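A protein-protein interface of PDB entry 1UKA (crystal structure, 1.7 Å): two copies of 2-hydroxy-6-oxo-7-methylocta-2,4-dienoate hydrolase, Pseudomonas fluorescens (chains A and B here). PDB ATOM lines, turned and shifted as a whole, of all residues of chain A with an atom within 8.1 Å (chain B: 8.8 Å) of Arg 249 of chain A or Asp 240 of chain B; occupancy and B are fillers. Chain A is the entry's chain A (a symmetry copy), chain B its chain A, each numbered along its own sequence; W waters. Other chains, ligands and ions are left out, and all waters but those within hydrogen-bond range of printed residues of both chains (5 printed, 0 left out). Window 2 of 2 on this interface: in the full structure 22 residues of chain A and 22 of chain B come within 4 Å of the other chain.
The guanidinium group (NH2) of Arg 222 of chain A is in salt-bridge range of the side-chain carboxylate (OD1) of Asp 240 of chain B (3.6 Å). The guanidinium group (NH2) of Arg 261 of chain A sits close to the side-chain amide nitrogen (NE2) of Gln 243 of chain B (3.4 Å). OD2 of Asp 240 of chain B is in salt-bridge range of NH1 of Arg 249 of chain A, 2.6 Å away. OE1 of Glu 215 of chain B lies within salt-bridge range of NH2 of Arg 261 of chain A, 3.0 Å away. The backbone carbonyl oxygen of Gly 236 of chain B sits at hydrogen-bond distance from the guanidinium group of Arg 222 of chain A (2.8 Å). NH1 of Arg 222 of chain A lies within hydrogen-bond range of O of Ile 239 of chain B (2.8 Å). O of Ala 242 of chain B sits at hydrogen-bond distance from N of Gly 248 of chain A (2.9 Å).
Of chain B, only Asp 240 and Arg 241 come within 4 Å of Arg 249 of chain A. Of chain A, only Arg 222 and Arg 249 come within 4 Å of Asp 240 of chain B. Of the printed residues of chain A, Gly 236 of chain B touches Arg 222 (2.8 Å). Printed residues of chain A within 4 Å of Ile 239 of chain B: Arg 222. Pro 213 of chain B touches none of the printed residues of chain A. The nearest residue of chain B that does not touch Arg 249 of chain A is Ala 242 of chain B (5.3 Å). The nearest printed residue of chain A that does not touch Asp 240 of chain B is Gly 248 of chain A (4.4 Å). The nearest printed residue of chain B that does not touch Arg 261 of chain A is Ala 242 of chain B (6.0 Å).
Of the 18 printed residues of chain A, 6 touch a printed residue of chain B. Hydrophobic or aromatic side chains of chain A within 4 Å of the printed part of chain B: Phe 247. Among the printed residues, 11 pairs touch across the chains. Among the printed residues, Asp or Glu carboxylates within 4 Å of a Lys or Arg side-chain nitrogen of the other chain: Arg 222 of chain A with Asp 240 of chain B (3.6 Å), Arg 249 of chain A with Asp 240 of chain B (2.6 Å) and Arg 261 of chain A with Glu 215 of chain B (3.0 Å).
Among the printed residues, merely in contact across the chains: Val 246 of chain A with Gln 243 of chain B (3.2 Å), Phe 247 of chain A with Gln 243 of chain B (3.3 Å), Arg 249 of chain A with Arg 241 of chain B (3.7 Å) and Arg 222 of chain A with Glu 237 of chain B (3.8 Å).
Water W4 bridges OH of Tyr 161 of chain A and OD1 of Asp 240 of chain B. Water W1 lies within hydrogen-bond range of the backbone carbonyl oxygen (O) of Glu 237 of chain B and the guanidinium group (NE) of Arg 222 of chain A. Water W2 bridges the backbone carbonyl oxygen of Arg 222 of chain A and the side-chain carboxylate of Glu 237 of chain B. Water W5 lies within hydrogen-bond range of OE2 of Glu 215 of chain B and NH2 of Arg 261 of chain A. Water W3 bridges the guanidinium group of Arg 241 of chain B (3.0 Å) and the guanidinium group of Arg 249 of chain A (3.5 Å).
No position is printed for both chains.
The side-chain hydroxyl (OH) of Tyr 161 of chain A lies within hydrogen-bond range of the guanidinium group (NH1) of Arg 249 of chain A (3.1 Å). The backbone carbonyl oxygen (O) of Phe 247 of chain A is in hydrogen-bond range of the backbone NH (N) of Arg 222 of chain A, at 2.9 Å. O of Thr 216 of chain B sits at hydrogen-bond distance from N of Gln 243 of chain B, 3.0 Å away. The backbone NH of Thr 216 of chain B lies within hydrogen-bond range of the backbone carbonyl oxygen of Arg 241 of chain B.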
ATOM      1  N   ALA A 160      22.722 -22.416  18.933  1.00  0.00           N
ATOM      2  CA  ALA A 160      21.335 -22.854  18.861  1.00  0.00           C
ATOM      3  C   ALA A 160      20.446 -22.263  17.784  1.00  0.00           C
ATOM      4  O   ALA A 160      20.573 -21.100  17.411  1.00  0.00           O
ATOM      5  CB  ALA A 160      20.671 -22.642  20.225  1.00  0.00           C
ATOM      6  N   TYR A 161      19.538 -23.093  17.288  1.00  0.00           N
ATOM      7  CA  TYR A 161      18.567 -22.645  16.308  1.00  0.00           C
ATOM      8  C   TYR A 161      17.429 -22.069  17.150  1.00  0.00           C
ATOM      9  O   TYR A 161      16.942 -20.963  16.901  1.00  0.00           O
ATOM     10  CB  TYR A 161      18.039 -23.819  15.485  1.00  0.00           C
ATOM     11  CG  TYR A 161      16.752 -23.481  14.781  1.00  0.00           C
ATOM     12  CD1 TYR A 161      16.743 -22.626  13.681  1.00  0.00           C
ATOM     13  CD2 TYR A 161      15.532 -23.955  15.262  1.00  0.00           C
ATOM     14  CE1 TYR A 161      15.544 -22.245  13.080  1.00  0.00           C
ATOM     15  CE2 TYR A 161      14.331 -23.580  14.671  1.00  0.00           C
ATOM     16  CZ  TYR A 161      14.344 -22.726  13.582  1.00  0.00           C
ATOM     17  OH  TYR A 161      13.153 -22.341  13.008  1.00  0.00           O
ATOM     18  N   ASP A 162      17.019 -22.841  18.152  1.00  0.00           N
ATOM     19  CA  ASP A 162      15.950 -22.441  19.064  1.00  0.00           C
ATOM     20  C   ASP A 162      16.585 -21.789  20.287  1.00  0.00           C
ATOM     21  O   ASP A 162      17.057 -22.480  21.192  1.00  0.00           O
ATOM     22  CB  ASP A 162      15.144 -23.661  19.511  1.00  0.00           C
ATOM     23  CG  ASP A 162      13.917 -23.283  20.323  1.00  0.00           C
ATOM     24  OD1 ASP A 162      13.943 -22.226  20.985  1.00  0.00           O
ATOM     25  OD2 ASP A 162      12.929 -24.048  20.308  1.00  0.00           O
ATOM     26  N   HIS A 220      24.939 -31.691   8.848  1.00  0.00           N
ATOM     27  CA  HIS A 220      25.043 -30.249   9.050  1.00  0.00           C
ATOM     28  C   HIS A 220      23.675 -29.638   9.337  1.00  0.00           C
ATOM     29  O   HIS A 220      22.657 -30.114   8.837  1.00  0.00           O
ATOM     30  CB  HIS A 220      25.633 -29.592   7.795  1.00  0.00           C
ATOM     31  CG  HIS A 220      26.460 -28.372   8.072  1.00  0.00           C
ATOM     32  ND1 HIS A 220      27.835 -28.376   7.992  1.00  0.00           N
ATOM     33  CD2 HIS A 220      26.108 -27.117   8.441  1.00  0.00           C
ATOM     34  CE1 HIS A 220      28.296 -27.174   8.296  1.00  0.00           C
ATOM     35  NE2 HIS A 220      27.268 -26.392   8.572  1.00  0.00           N
ATOM     36  N   GLY A 221      23.665 -28.594  10.162  1.00  0.00           N
ATOM     37  CA  GLY A 221      22.431 -27.895  10.475  1.00  0.00           C
ATOM     38  C   GLY A 221      22.315 -26.752   9.483  1.00  0.00           C
ATOM     39  O   GLY A 221      23.255 -25.982   9.305  1.00  0.00           O
ATOM     40  N   ARG A 222      21.165 -26.632   8.832  1.00  0.00           N
ATOM     41  CA  ARG A 222      20.970 -25.590   7.830  1.00  0.00           C
ATOM     42  C   ARG A 222      21.350 -24.197   8.320  1.00  0.00           C
ATOM     43  O   ARG A 222      22.035 -23.442   7.623  1.00  0.00           O
ATOM     44  CB  ARG A 222      19.511 -25.589   7.363  1.00  0.00           C
ATOM     45  CG  ARG A 222      19.195 -24.570   6.277  1.00  0.00           C
ATOM     46  CD  ARG A 222      17.766 -24.747   5.780  1.00  0.00           C
ATOM     47  NE  ARG A 222      16.785 -24.484   6.832  1.00  0.00           N
ATOM     48  CZ  ARG A 222      15.504 -24.831   6.763  1.00  0.00           C
ATOM     49  NH1 ARG A 222      15.044 -25.464   5.690  1.00  0.00           N
ATOM     50  NH2 ARG A 222      14.679 -24.541   7.762  1.00  0.00           N
ATOM     51  N   GLU A 223      20.913 -23.873   9.529  1.00  0.00           N
ATOM     52  CA  GLU A 223      21.155 -22.562  10.115  1.00  0.00           C
ATOM     53  C   GLU A 223      22.480 -22.389  10.866  1.00  0.00           C
ATOM     54  O   GLU A 223      22.675 -21.382  11.546  1.00  0.00           O
ATOM     55  CB  GLU A 223      19.992 -22.207  11.049  1.00  0.00           C
ATOM     56  CG  GLU A 223      18.642 -21.972  10.352  1.00  0.00           C
ATOM     57  CD  GLU A 223      17.887 -23.250  10.001  1.00  0.00           C
ATOM     58  OE1 GLU A 223      18.336 -24.353  10.381  1.00  0.00           O
ATOM     59  OE2 GLU A 223      16.825 -23.145   9.348  1.00  0.00           O
ATOM     60  N   ASP A 224      23.387 -23.354  10.741  1.00  0.00           N
ATOM     61  CA  ASP A 224      24.680 -23.282  11.427  1.00  0.00           C
ATOM     62  C   ASP A 224      25.341 -21.914  11.215  1.00  0.00           C
ATOM     63  O   ASP A 224      25.613 -21.517  10.078  1.00  0.00           O
ATOM     64  CB  ASP A 224      25.607 -24.384  10.907  1.00  0.00           C
ATOM     65  CG  ASP A 224      26.795 -24.636  11.820  1.00  0.00           C
ATOM     66  OD1 ASP A 224      27.323 -23.669  12.417  1.00  0.00           O
ATOM     67  OD2 ASP A 224      27.214 -25.808  11.927  1.00  0.00           O
ATOM     68  N   VAL A 246      21.293 -32.835   5.811  1.00  0.00           N
ATOM     69  CA  VAL A 246      21.144 -31.488   6.335  1.00  0.00           C
ATOM     70  C   VAL A 246      19.840 -31.389   7.110  1.00  0.00           C
ATOM     71  O   VAL A 246      18.774 -31.723   6.595  1.00  0.00           O
ATOM     72  CB  VAL A 246      21.130 -30.449   5.193  1.00  0.00           C
ATOM     73  CG1 VAL A 246      20.973 -29.043   5.764  1.00  0.00           C
ATOM     74  CG2 VAL A 246      22.418 -30.551   4.387  1.00  0.00           C
ATOM     75  N   PHE A 247      19.939 -30.943   8.357  1.00  0.00           N
ATOM     76  CA  PHE A 247      18.769 -30.778   9.211  1.00  0.00           C
ATOM     77  C   PHE A 247      18.302 -29.330   9.181  1.00  0.00           C
ATOM     78  O   PHE A 247      19.053 -28.424   9.553  1.00  0.00           O
ATOM     79  CB  PHE A 247      19.097 -31.117  10.669  1.00  0.00           C
ATOM     80  CG  PHE A 247      19.339 -32.574  10.933  1.00  0.00           C
ATOM     81  CD1 PHE A 247      18.318 -33.509  10.782  1.00  0.00           C
ATOM     82  CD2 PHE A 247      20.575 -33.005  11.401  1.00  0.00           C
ATOM     83  CE1 PHE A 247      18.526 -34.849  11.101  1.00  0.00           C
ATOM     84  CE2 PHE A 247      20.794 -34.340  11.721  1.00  0.00           C
ATOM     85  CZ  PHE A 247      19.767 -35.266  11.573  1.00  0.00           C
ATOM     86  N   GLY A 248      17.070 -29.109   8.738  1.00  0.00           N
ATOM     87  CA  GLY A 248      16.536 -27.762   8.748  1.00  0.00           C
ATOM     88  C   GLY A 248      16.172 -27.469  10.195  1.00  0.00           C
ATOM     89  O   GLY A 248      15.988 -28.402  10.982  1.00  0.00           O
ATOM     90  N   ARG A 249      16.072 -26.190  10.552  1.00  0.00           N
ATOM     91  CA  ARG A 249      15.738 -25.793  11.918  1.00  0.00           C
ATOM     92  C   ARG A 249      16.732 -26.430  12.879  1.00  0.00           C
ATOM     93  O   ARG A 249      16.361 -27.061  13.871  1.00  0.00           O
ATOM     94  CB  ARG A 249      14.307 -26.226  12.263  1.00  0.00           C
ATOM     95  CG  ARG A 249      13.242 -25.580  11.384  1.00  0.00           C
ATOM     96  CD  ARG A 249      11.862 -26.162  11.672  1.00  0.00           C
ATOM     97  NE  ARG A 249      11.397 -25.827  13.014  1.00  0.00           N
ATOM     98  CZ  ARG A 249      10.738 -24.715  13.326  1.00  0.00           C
ATOM     99  NH1 ARG A 249      10.454 -23.820  12.389  1.00  0.00           N
ATOM    100  NH2 ARG A 249      10.370 -24.494  14.580  1.00  0.00           N
ATOM    101  N   CYS A 250      18.011 -26.248  12.576  1.00  0.00           N
ATOM    102  CA  CYS A 250      19.063 -26.823  13.393  1.00  0.00           C
ATOM    103  C   CYS A 250      20.339 -26.008  13.266  1.00  0.00           C
ATOM    104  O   CYS A 250      20.729 -25.622  12.162  1.00  0.00           O
ATOM    105  CB  CYS A 250      19.315 -28.263  12.952  1.00  0.00           C
ATOM    106  SG  CYS A 250      20.527 -29.137  13.948  1.00  0.00           S
ATOM    107  N   GLY A 251      20.977 -25.757  14.404  1.00  0.00           N
ATOM    108  CA  GLY A 251      22.198 -24.978  14.427  1.00  0.00           C
ATOM    109  C   GLY A 251      23.480 -25.785  14.368  1.00  0.00           C
ATOM    110  O   GLY A 251      23.552 -26.823  13.704  1.00  0.00           O
ATOM    111  N   THR A 254      24.018 -30.321  16.184  1.00  0.00           N
ATOM    112  CA  THR A 254      22.963 -31.207  15.734  1.00  0.00           C
ATOM    113  C   THR A 254      22.684 -32.361  16.686  1.00  0.00           C
ATOM    114  O   THR A 254      21.560 -32.846  16.745  1.00  0.00           O
ATOM    115  CB  THR A 254      23.300 -31.786  14.346  1.00  0.00           C
ATOM    116  OG1 THR A 254      24.498 -32.572  14.431  1.00  0.00           O
ATOM    117  CG2 THR A 254      23.523 -30.660  13.343  1.00  0.00           C
ATOM    118  N   GLU A 257      20.149 -30.566  19.251  1.00  0.00           N
ATOM    119  CA  GLU A 257      18.861 -30.089  18.754  1.00  0.00           C
ATOM    120  C   GLU A 257      18.082 -31.052  17.865  1.00  0.00           C
ATOM    121  O   GLU A 257      16.898 -30.841  17.604  1.00  0.00           O
ATOM    122  CB  GLU A 257      19.039 -28.755  18.029  1.00  0.00           C
ATOM    123  CG  GLU A 257      19.089 -27.572  18.976  1.00  0.00           C
ATOM    124  CD  GLU A 257      18.984 -26.249  18.252  1.00  0.00           C
ATOM    125  OE1 GLU A 257      19.959 -25.864  17.574  1.00  0.00           O
ATOM    126  OE2 GLU A 257      17.921 -25.602  18.355  1.00  0.00           O
ATOM    127  N   GLN A 258      18.748 -32.098  17.392  1.00  0.00           N
ATOM    128  CA  GLN A 258      18.109 -33.112  16.556  1.00  0.00           C
ATOM    129  C   GLN A 258      18.630 -34.450  17.071  1.00  0.00           C
ATOM    130  O   GLN A 258      18.924 -35.363  16.302  1.00  0.00           O
ATOM    131  CB  GLN A 258      18.496 -32.917  15.089  1.00  0.00           C
ATOM    132  CG  GLN A 258      17.986 -31.617  14.468  1.00  0.00           C
ATOM    133  CD  GLN A 258      16.506 -31.661  14.129  1.00  0.00           C
ATOM    134  OE1 GLN A 258      16.076 -32.433  13.272  1.00  0.00           O
ATOM    135  NE2 GLN A 258      15.719 -30.830  14.800  1.00  0.00           N
ATOM    136  N   ARG A 261      16.973 -37.942  15.893  1.00  0.00           N
ATOM    137  CA  ARG A 261      17.224 -38.145  14.469  1.00  0.00           C
ATOM    138  C   ARG A 261      18.709 -38.429  14.232  1.00  0.00           C
ATOM    139  O   ARG A 261      19.072 -39.317  13.460  1.00  0.00           O
ATOM    140  CB  ARG A 261      16.811 -36.905  13.677  1.00  0.00           C
ATOM    141  CG  ARG A 261      15.312 -36.758  13.517  1.00  0.00           C
ATOM    142  CD  ARG A 261      14.968 -35.435  12.864  1.00  0.00           C
ATOM    143  NE  ARG A 261      13.564 -35.379  12.466  1.00  0.00           N
ATOM    144  CZ  ARG A 261      12.983 -34.304  11.945  1.00  0.00           C
ATOM    145  NH1 ARG A 261      13.685 -33.193  11.765  1.00  0.00           N
ATOM    146  NH2 ARG A 261      11.708 -34.348  11.579  1.00  0.00           N
ATOM    147  N   ILE B 209       6.113 -22.245  -2.048  1.00  0.00           N
ATOM    148  CA  ILE B 209       6.839 -23.329  -1.403  1.00  0.00           C
ATOM    149  C   ILE B 209       7.207 -22.972   0.034  1.00  0.00           C
ATOM    150  O   ILE B 209       7.160 -23.823   0.925  1.00  0.00           O
ATOM    151  CB  ILE B 209       8.110 -23.691  -2.207  1.00  0.00           C
ATOM    152  CG1 ILE B 209       7.697 -24.257  -3.571  1.00  0.00           C
ATOM    153  CG2 ILE B 209       8.958 -24.710  -1.439  1.00  0.00           C
ATOM    154  CD1 ILE B 209       8.854 -24.597  -4.483  1.00  0.00           C
ATOM    155  N   LYS B 210       7.559 -21.712   0.264  1.00  0.00           N
ATOM    156  CA  LYS B 210       7.925 -21.270   1.605  1.00  0.00           C
ATOM    157  C   LYS B 210       6.771 -21.377   2.594  1.00  0.00           C
ATOM    158  O   LYS B 210       6.997 -21.394   3.802  1.00  0.00           O
ATOM    159  CB  LYS B 210       8.427 -19.822   1.579  1.00  0.00           C
ATOM    160  CG  LYS B 210       9.785 -19.630   0.934  1.00  0.00           C
ATOM    161  CD  LYS B 210      10.156 -18.154   0.932  1.00  0.00           C
ATOM    162  CE  LYS B 210      11.495 -17.911   0.268  1.00  0.00           C
ATOM    163  NZ  LYS B 210      11.815 -16.456   0.222  1.00  0.00           N
ATOM    164  N   THR B 211       5.537 -21.447   2.093  1.00  0.00           N
ATOM    165  CA  THR B 211       4.375 -21.543   2.976  1.00  0.00           C
ATOM    166  C   THR B 211       4.058 -22.967   3.427  1.00  0.00           C
ATOM    167  O   THR B 211       3.216 -23.166   4.306  1.00  0.00           O
ATOM    168  CB  THR B 211       3.095 -20.971   2.317  1.00  0.00           C
ATOM    169  OG1 THR B 211       2.662 -21.840   1.262  1.00  0.00           O
ATOM    170  CG2 THR B 211       3.355 -19.582   1.758  1.00  0.00           C
ATOM    171  N   LEU B 212       4.720 -23.955   2.832  1.00  0.00           N
ATOM    172  CA  LEU B 212       4.474 -25.352   3.195  1.00  0.00           C
ATOM    173  C   LEU B 212       4.807 -25.614   4.661  1.00  0.00           C
ATOM    174  O   LEU B 212       5.937 -25.404   5.097  1.00  0.00           O
ATOM    175  CB  LEU B 212       5.297 -26.284   2.308  1.00  0.00           C
ATOM    176  CG  LEU B 212       4.834 -26.394   0.855  1.00  0.00           C
ATOM    177  CD1 LEU B 212       5.867 -27.168   0.050  1.00  0.00           C
ATOM    178  CD2 LEU B 212       3.475 -27.079   0.804  1.00  0.00           C
ATOM    179  N   PRO B 213       3.821 -26.089   5.439  1.00  0.00           N
ATOM    180  CA  PRO B 213       4.025 -26.372   6.862  1.00  0.00           C
ATOM    181  C   PRO B 213       4.445 -27.808   7.157  1.00  0.00           C
ATOM    182  O   PRO B 213       4.843 -28.126   8.278  1.00  0.00           O
ATOM    183  CB  PRO B 213       2.661 -26.062   7.454  1.00  0.00           C
ATOM    184  CG  PRO B 213       1.746 -26.626   6.401  1.00  0.00           C
ATOM    185  CD  PRO B 213       2.385 -26.144   5.098  1.00  0.00           C
ATOM    186  N   ASN B 214       4.367 -28.658   6.140  1.00  0.00           N
ATOM    187  CA  ASN B 214       4.676 -30.080   6.274  1.00  0.00           C
ATOM    188  C   ASN B 214       6.112 -30.466   6.581  1.00  0.00           C
ATOM    189  O   ASN B 214       7.049 -29.868   6.052  1.00  0.00           O
ATOM    190  CB  ASN B 214       4.292 -30.830   4.993  1.00  0.00           C
ATOM    191  CG  ASN B 214       3.038 -30.291   4.346  1.00  0.00           C
ATOM    192  OD1 ASN B 214       3.026 -29.177   3.821  1.00  0.00           O
ATOM    193  ND2 ASN B 214       1.972 -31.083   4.375  1.00  0.00           N
ATOM    194  N   GLU B 215       6.275 -31.475   7.437  1.00  0.00           N
ATOM    195  CA  GLU B 215       7.602 -32.008   7.727  1.00  0.00           C
ATOM    196  C   GLU B 215       7.935 -32.638   6.378  1.00  0.00           C
ATOM    197  O   GLU B 215       7.137 -33.415   5.836  1.00  0.00           O
ATOM    198  CB  GLU B 215       7.546 -33.105   8.796  1.00  0.00           C
ATOM    199  CG  GLU B 215       7.544 -32.626  10.245  1.00  0.00           C
ATOM    200  CD  GLU B 215       8.884 -32.062  10.697  1.00  0.00           C
ATOM    201  OE1 GLU B 215       9.933 -32.462  10.148  1.00  0.00           O
ATOM    202  OE2 GLU B 215       8.890 -31.226  11.623  1.00  0.00           O
ATOM    203  N   THR B 216       9.101 -32.308   5.836  1.00  0.00           N
ATOM    204  CA  THR B 216       9.482 -32.804   4.522  1.00  0.00           C
ATOM    205  C   THR B 216      10.885 -33.390   4.496  1.00  0.00           C
ATOM    206  O   THR B 216      11.790 -32.893   5.163  1.00  0.00           O
ATOM    207  CB  THR B 216       9.408 -31.653   3.484  1.00  0.00           C
ATOM    208  OG1 THR B 216       8.112 -31.044   3.540  1.00  0.00           O
ATOM    209  CG2 THR B 216       9.660 -32.166   2.074  1.00  0.00           C
ATOM    210  N   ILE B 218      13.742 -34.316   1.748  1.00  0.00           N
ATOM    211  CA  ILE B 218      14.168 -34.136   0.364  1.00  0.00           C
ATOM    212  C   ILE B 218      15.340 -35.074   0.106  1.00  0.00           C
ATOM    213  O   ILE B 218      16.341 -35.028   0.814  1.00  0.00           O
ATOM    214  CB  ILE B 218      14.606 -32.680   0.125  1.00  0.00           C
ATOM    215  CG1 ILE B 218      13.484 -31.729   0.555  1.00  0.00           C
ATOM    216  CG2 ILE B 218      14.937 -32.467  -1.346  1.00  0.00           C
ATOM    217  CD1 ILE B 218      13.930 -30.284   0.692  1.00  0.00           C
ATOM    218  N   ARG B 234      17.863 -26.090  -3.358  1.00  0.00           N
ATOM    219  CA  ARG B 234      16.974 -24.938  -3.331  1.00  0.00           C
ATOM    220  C   ARG B 234      15.728 -25.278  -2.518  1.00  0.00           C
ATOM    221  O   ARG B 234      15.286 -24.486  -1.687  1.00  0.00           O
ATOM    222  CB  ARG B 234      16.585 -24.531  -4.757  1.00  0.00           C
ATOM    223  CG  ARG B 234      15.706 -23.288  -4.835  1.00  0.00           C
ATOM    224  CD  ARG B 234      16.341 -22.115  -4.101  1.00  0.00           C
ATOM    225  NE  ARG B 234      15.575 -20.881  -4.267  1.00  0.00           N
ATOM    226  CZ  ARG B 234      15.800 -19.765  -3.582  1.00  0.00           C
ATOM    227  NH1 ARG B 234      16.771 -19.722  -2.678  1.00  0.00           N
ATOM    228  NH2 ARG B 234      15.053 -18.690  -3.801  1.00  0.00           N
ATOM    229  N   LEU B 235      15.156 -26.454  -2.758  1.00  0.00           N
ATOM    230  CA  LEU B 235      13.980 -26.869  -2.002  1.00  0.00           C
ATOM    231  C   LEU B 235      14.328 -26.942  -0.515  1.00  0.00           C
ATOM    232  O   LEU B 235      13.501 -26.625   0.341  1.00  0.00           O
ATOM    233  CB  LEU B 235      13.487 -28.239  -2.482  1.00  0.00           C
ATOM    234  CG  LEU B 235      12.826 -28.285  -3.860  1.00  0.00           C
ATOM    235  CD1 LEU B 235      12.532 -29.732  -4.242  1.00  0.00           C
ATOM    236  CD2 LEU B 235      11.536 -27.470  -3.834  1.00  0.00           C
ATOM    237  N   GLY B 236      15.556 -27.355  -0.217  1.00  0.00           N
ATOM    238  CA  GLY B 236      15.994 -27.469   1.165  1.00  0.00           C
ATOM    239  C   GLY B 236      16.092 -26.136   1.881  1.00  0.00           C
ATOM    240  O   GLY B 236      16.034 -26.078   3.109  1.00  0.00           O
ATOM    241  N   GLU B 237      16.248 -25.064   1.114  1.00  0.00           N
ATOM    242  CA  GLU B 237      16.345 -23.727   1.687  1.00  0.00           C
ATOM    243  C   GLU B 237      14.968 -23.079   1.790  1.00  0.00           C
ATOM    244  O   GLU B 237      14.730 -22.246   2.663  1.00  0.00           O
ATOM    245  CB  GLU B 237      17.252 -22.844   0.828  1.00  0.00           C
ATOM    246  CG  GLU B 237      18.738 -23.156   0.924  1.00  0.00           C
ATOM    247  CD  GLU B 237      19.285 -22.983   2.332  1.00  0.00           C
ATOM    248  OE1 GLU B 237      18.801 -22.086   3.056  1.00  0.00           O
ATOM    249  OE2 GLU B 237      20.210 -23.733   2.711  1.00  0.00           O
ATOM    250  N   LEU B 238      14.064 -23.472   0.896  1.00  0.00           N
ATOM    251  CA  LEU B 238      12.713 -22.919   0.857  1.00  0.00           C
ATOM    252  C   LEU B 238      11.735 -23.523   1.866  1.00  0.00           C
ATOM    253  O   LEU B 238      10.976 -22.797   2.507  1.00  0.00           O
ATOM    254  CB  LEU B 238      12.129 -23.083  -0.550  1.00  0.00           C
ATOM    255  CG  LEU B 238      12.815 -22.313  -1.680  1.00  0.00           C
ATOM    256  CD1 LEU B 238      12.260 -22.776  -3.017  1.00  0.00           C
ATOM    257  CD2 LEU B 238      12.594 -20.817  -1.494  1.00  0.00           C
ATOM    258  N   ILE B 239      11.740 -24.847   1.993  1.00  0.00           N
ATOM    259  CA  ILE B 239      10.827 -25.521   2.913  1.00  0.00           C
ATOM    260  C   ILE B 239      11.375 -25.475   4.338  1.00  0.00           C
ATOM    261  O   ILE B 239      12.476 -25.953   4.609  1.00  0.00           O
ATOM    262  CB  ILE B 239      10.588 -26.980   2.463  1.00  0.00           C
ATOM    263  CG1 ILE B 239       9.965 -26.981   1.061  1.00  0.00           C
ATOM    264  CG2 ILE B 239       9.664 -27.693   3.444  1.00  0.00           C
ATOM    265  CD1 ILE B 239       9.766 -28.375   0.470  1.00  0.00           C
ATOM    266  N   ASP B 240      10.595 -24.903   5.250  1.00  0.00           N
ATOM    267  CA  ASP B 240      11.040 -24.758   6.632  1.00  0.00           C
ATOM    268  C   ASP B 240      11.345 -26.054   7.375  1.00  0.00           C
ATOM    269  O   ASP B 240      12.473 -26.259   7.822  1.00  0.00           O
ATOM    270  CB  ASP B 240      10.030 -23.938   7.434  1.00  0.00           C
ATOM    271  CG  ASP B 240      10.557 -23.562   8.805  1.00  0.00           C
ATOM    272  OD1 ASP B 240      11.671 -23.000   8.875  1.00  0.00           O
ATOM    273  OD2 ASP B 240       9.867 -23.827   9.808  1.00  0.00           O
ATOM    274  N   ARG B 241      10.351 -26.921   7.531  1.00  0.00           N
ATOM    275  CA  ARG B 241      10.581 -28.176   8.242  1.00  0.00           C
ATOM    276  C   ARG B 241      11.132 -29.233   7.299  1.00  0.00           C
ATOM    277  O   ARG B 241      10.534 -30.292   7.113  1.00  0.00           O
ATOM    278  CB  ARG B 241       9.284 -28.667   8.886  1.00  0.00           C
ATOM    279  CG  ARG B 241       8.797 -27.779  10.020  1.00  0.00           C
ATOM    280  CD  ARG B 241       7.530 -28.324  10.659  1.00  0.00           C
ATOM    281  NE  ARG B 241       7.165 -27.572  11.856  1.00  0.00           N
ATOM    282  CZ  ARG B 241       7.804 -27.652  13.019  1.00  0.00           C
ATOM    283  NH1 ARG B 241       8.849 -28.458  13.156  1.00  0.00           N
ATOM    284  NH2 ARG B 241       7.403 -26.916  14.048  1.00  0.00           N
ATOM    285  N   ALA B 242      12.293 -28.953   6.722  1.00  0.00           N
ATOM    286  CA  ALA B 242      12.880 -29.886   5.779  1.00  0.00           C
ATOM    287  C   ALA B 242      14.217 -30.474   6.188  1.00  0.00           C
ATOM    288  O   ALA B 242      14.990 -29.872   6.929  1.00  0.00           O
ATOM    289  CB  ALA B 242      13.028 -29.211   4.422  1.00  0.00           C
ATOM    290  N   GLN B 243      14.458 -31.681   5.694  1.00  0.00           N
ATOM    291  CA  GLN B 243      15.715 -32.376   5.893  1.00  0.00           C
ATOM    292  C   GLN B 243      16.124 -32.723   4.473  1.00  0.00           C
ATOM    293  O   GLN B 243      15.275 -33.056   3.645  1.00  0.00           O
ATOM    294  CB  GLN B 243      15.535 -33.673   6.673  1.00  0.00           C
ATOM    295  CG  GLN B 243      15.162 -33.508   8.123  1.00  0.00           C
ATOM    296  CD  GLN B 243      14.997 -34.849   8.798  1.00  0.00           C
ATOM    297  OE1 GLN B 243      15.979 -35.535   9.097  1.00  0.00           O
ATOM    298  NE2 GLN B 243      13.751 -35.246   9.023  1.00  0.00           N
HETATM  299  O   HOH W   1      15.356 -21.836   5.290  1.00  0.00           O
HETATM  300  O   HOH W   2      21.757 -22.287   5.135  1.00  0.00           O
HETATM  301  O   HOH W   3       9.692 -27.594  15.940  1.00  0.00           O
HETATM  302  O   HOH W   4      12.983 -21.634  10.595  1.00  0.00           O
HETATM  303  O   HOH W   5      10.002 -32.559  14.023  1.00  0.00           O
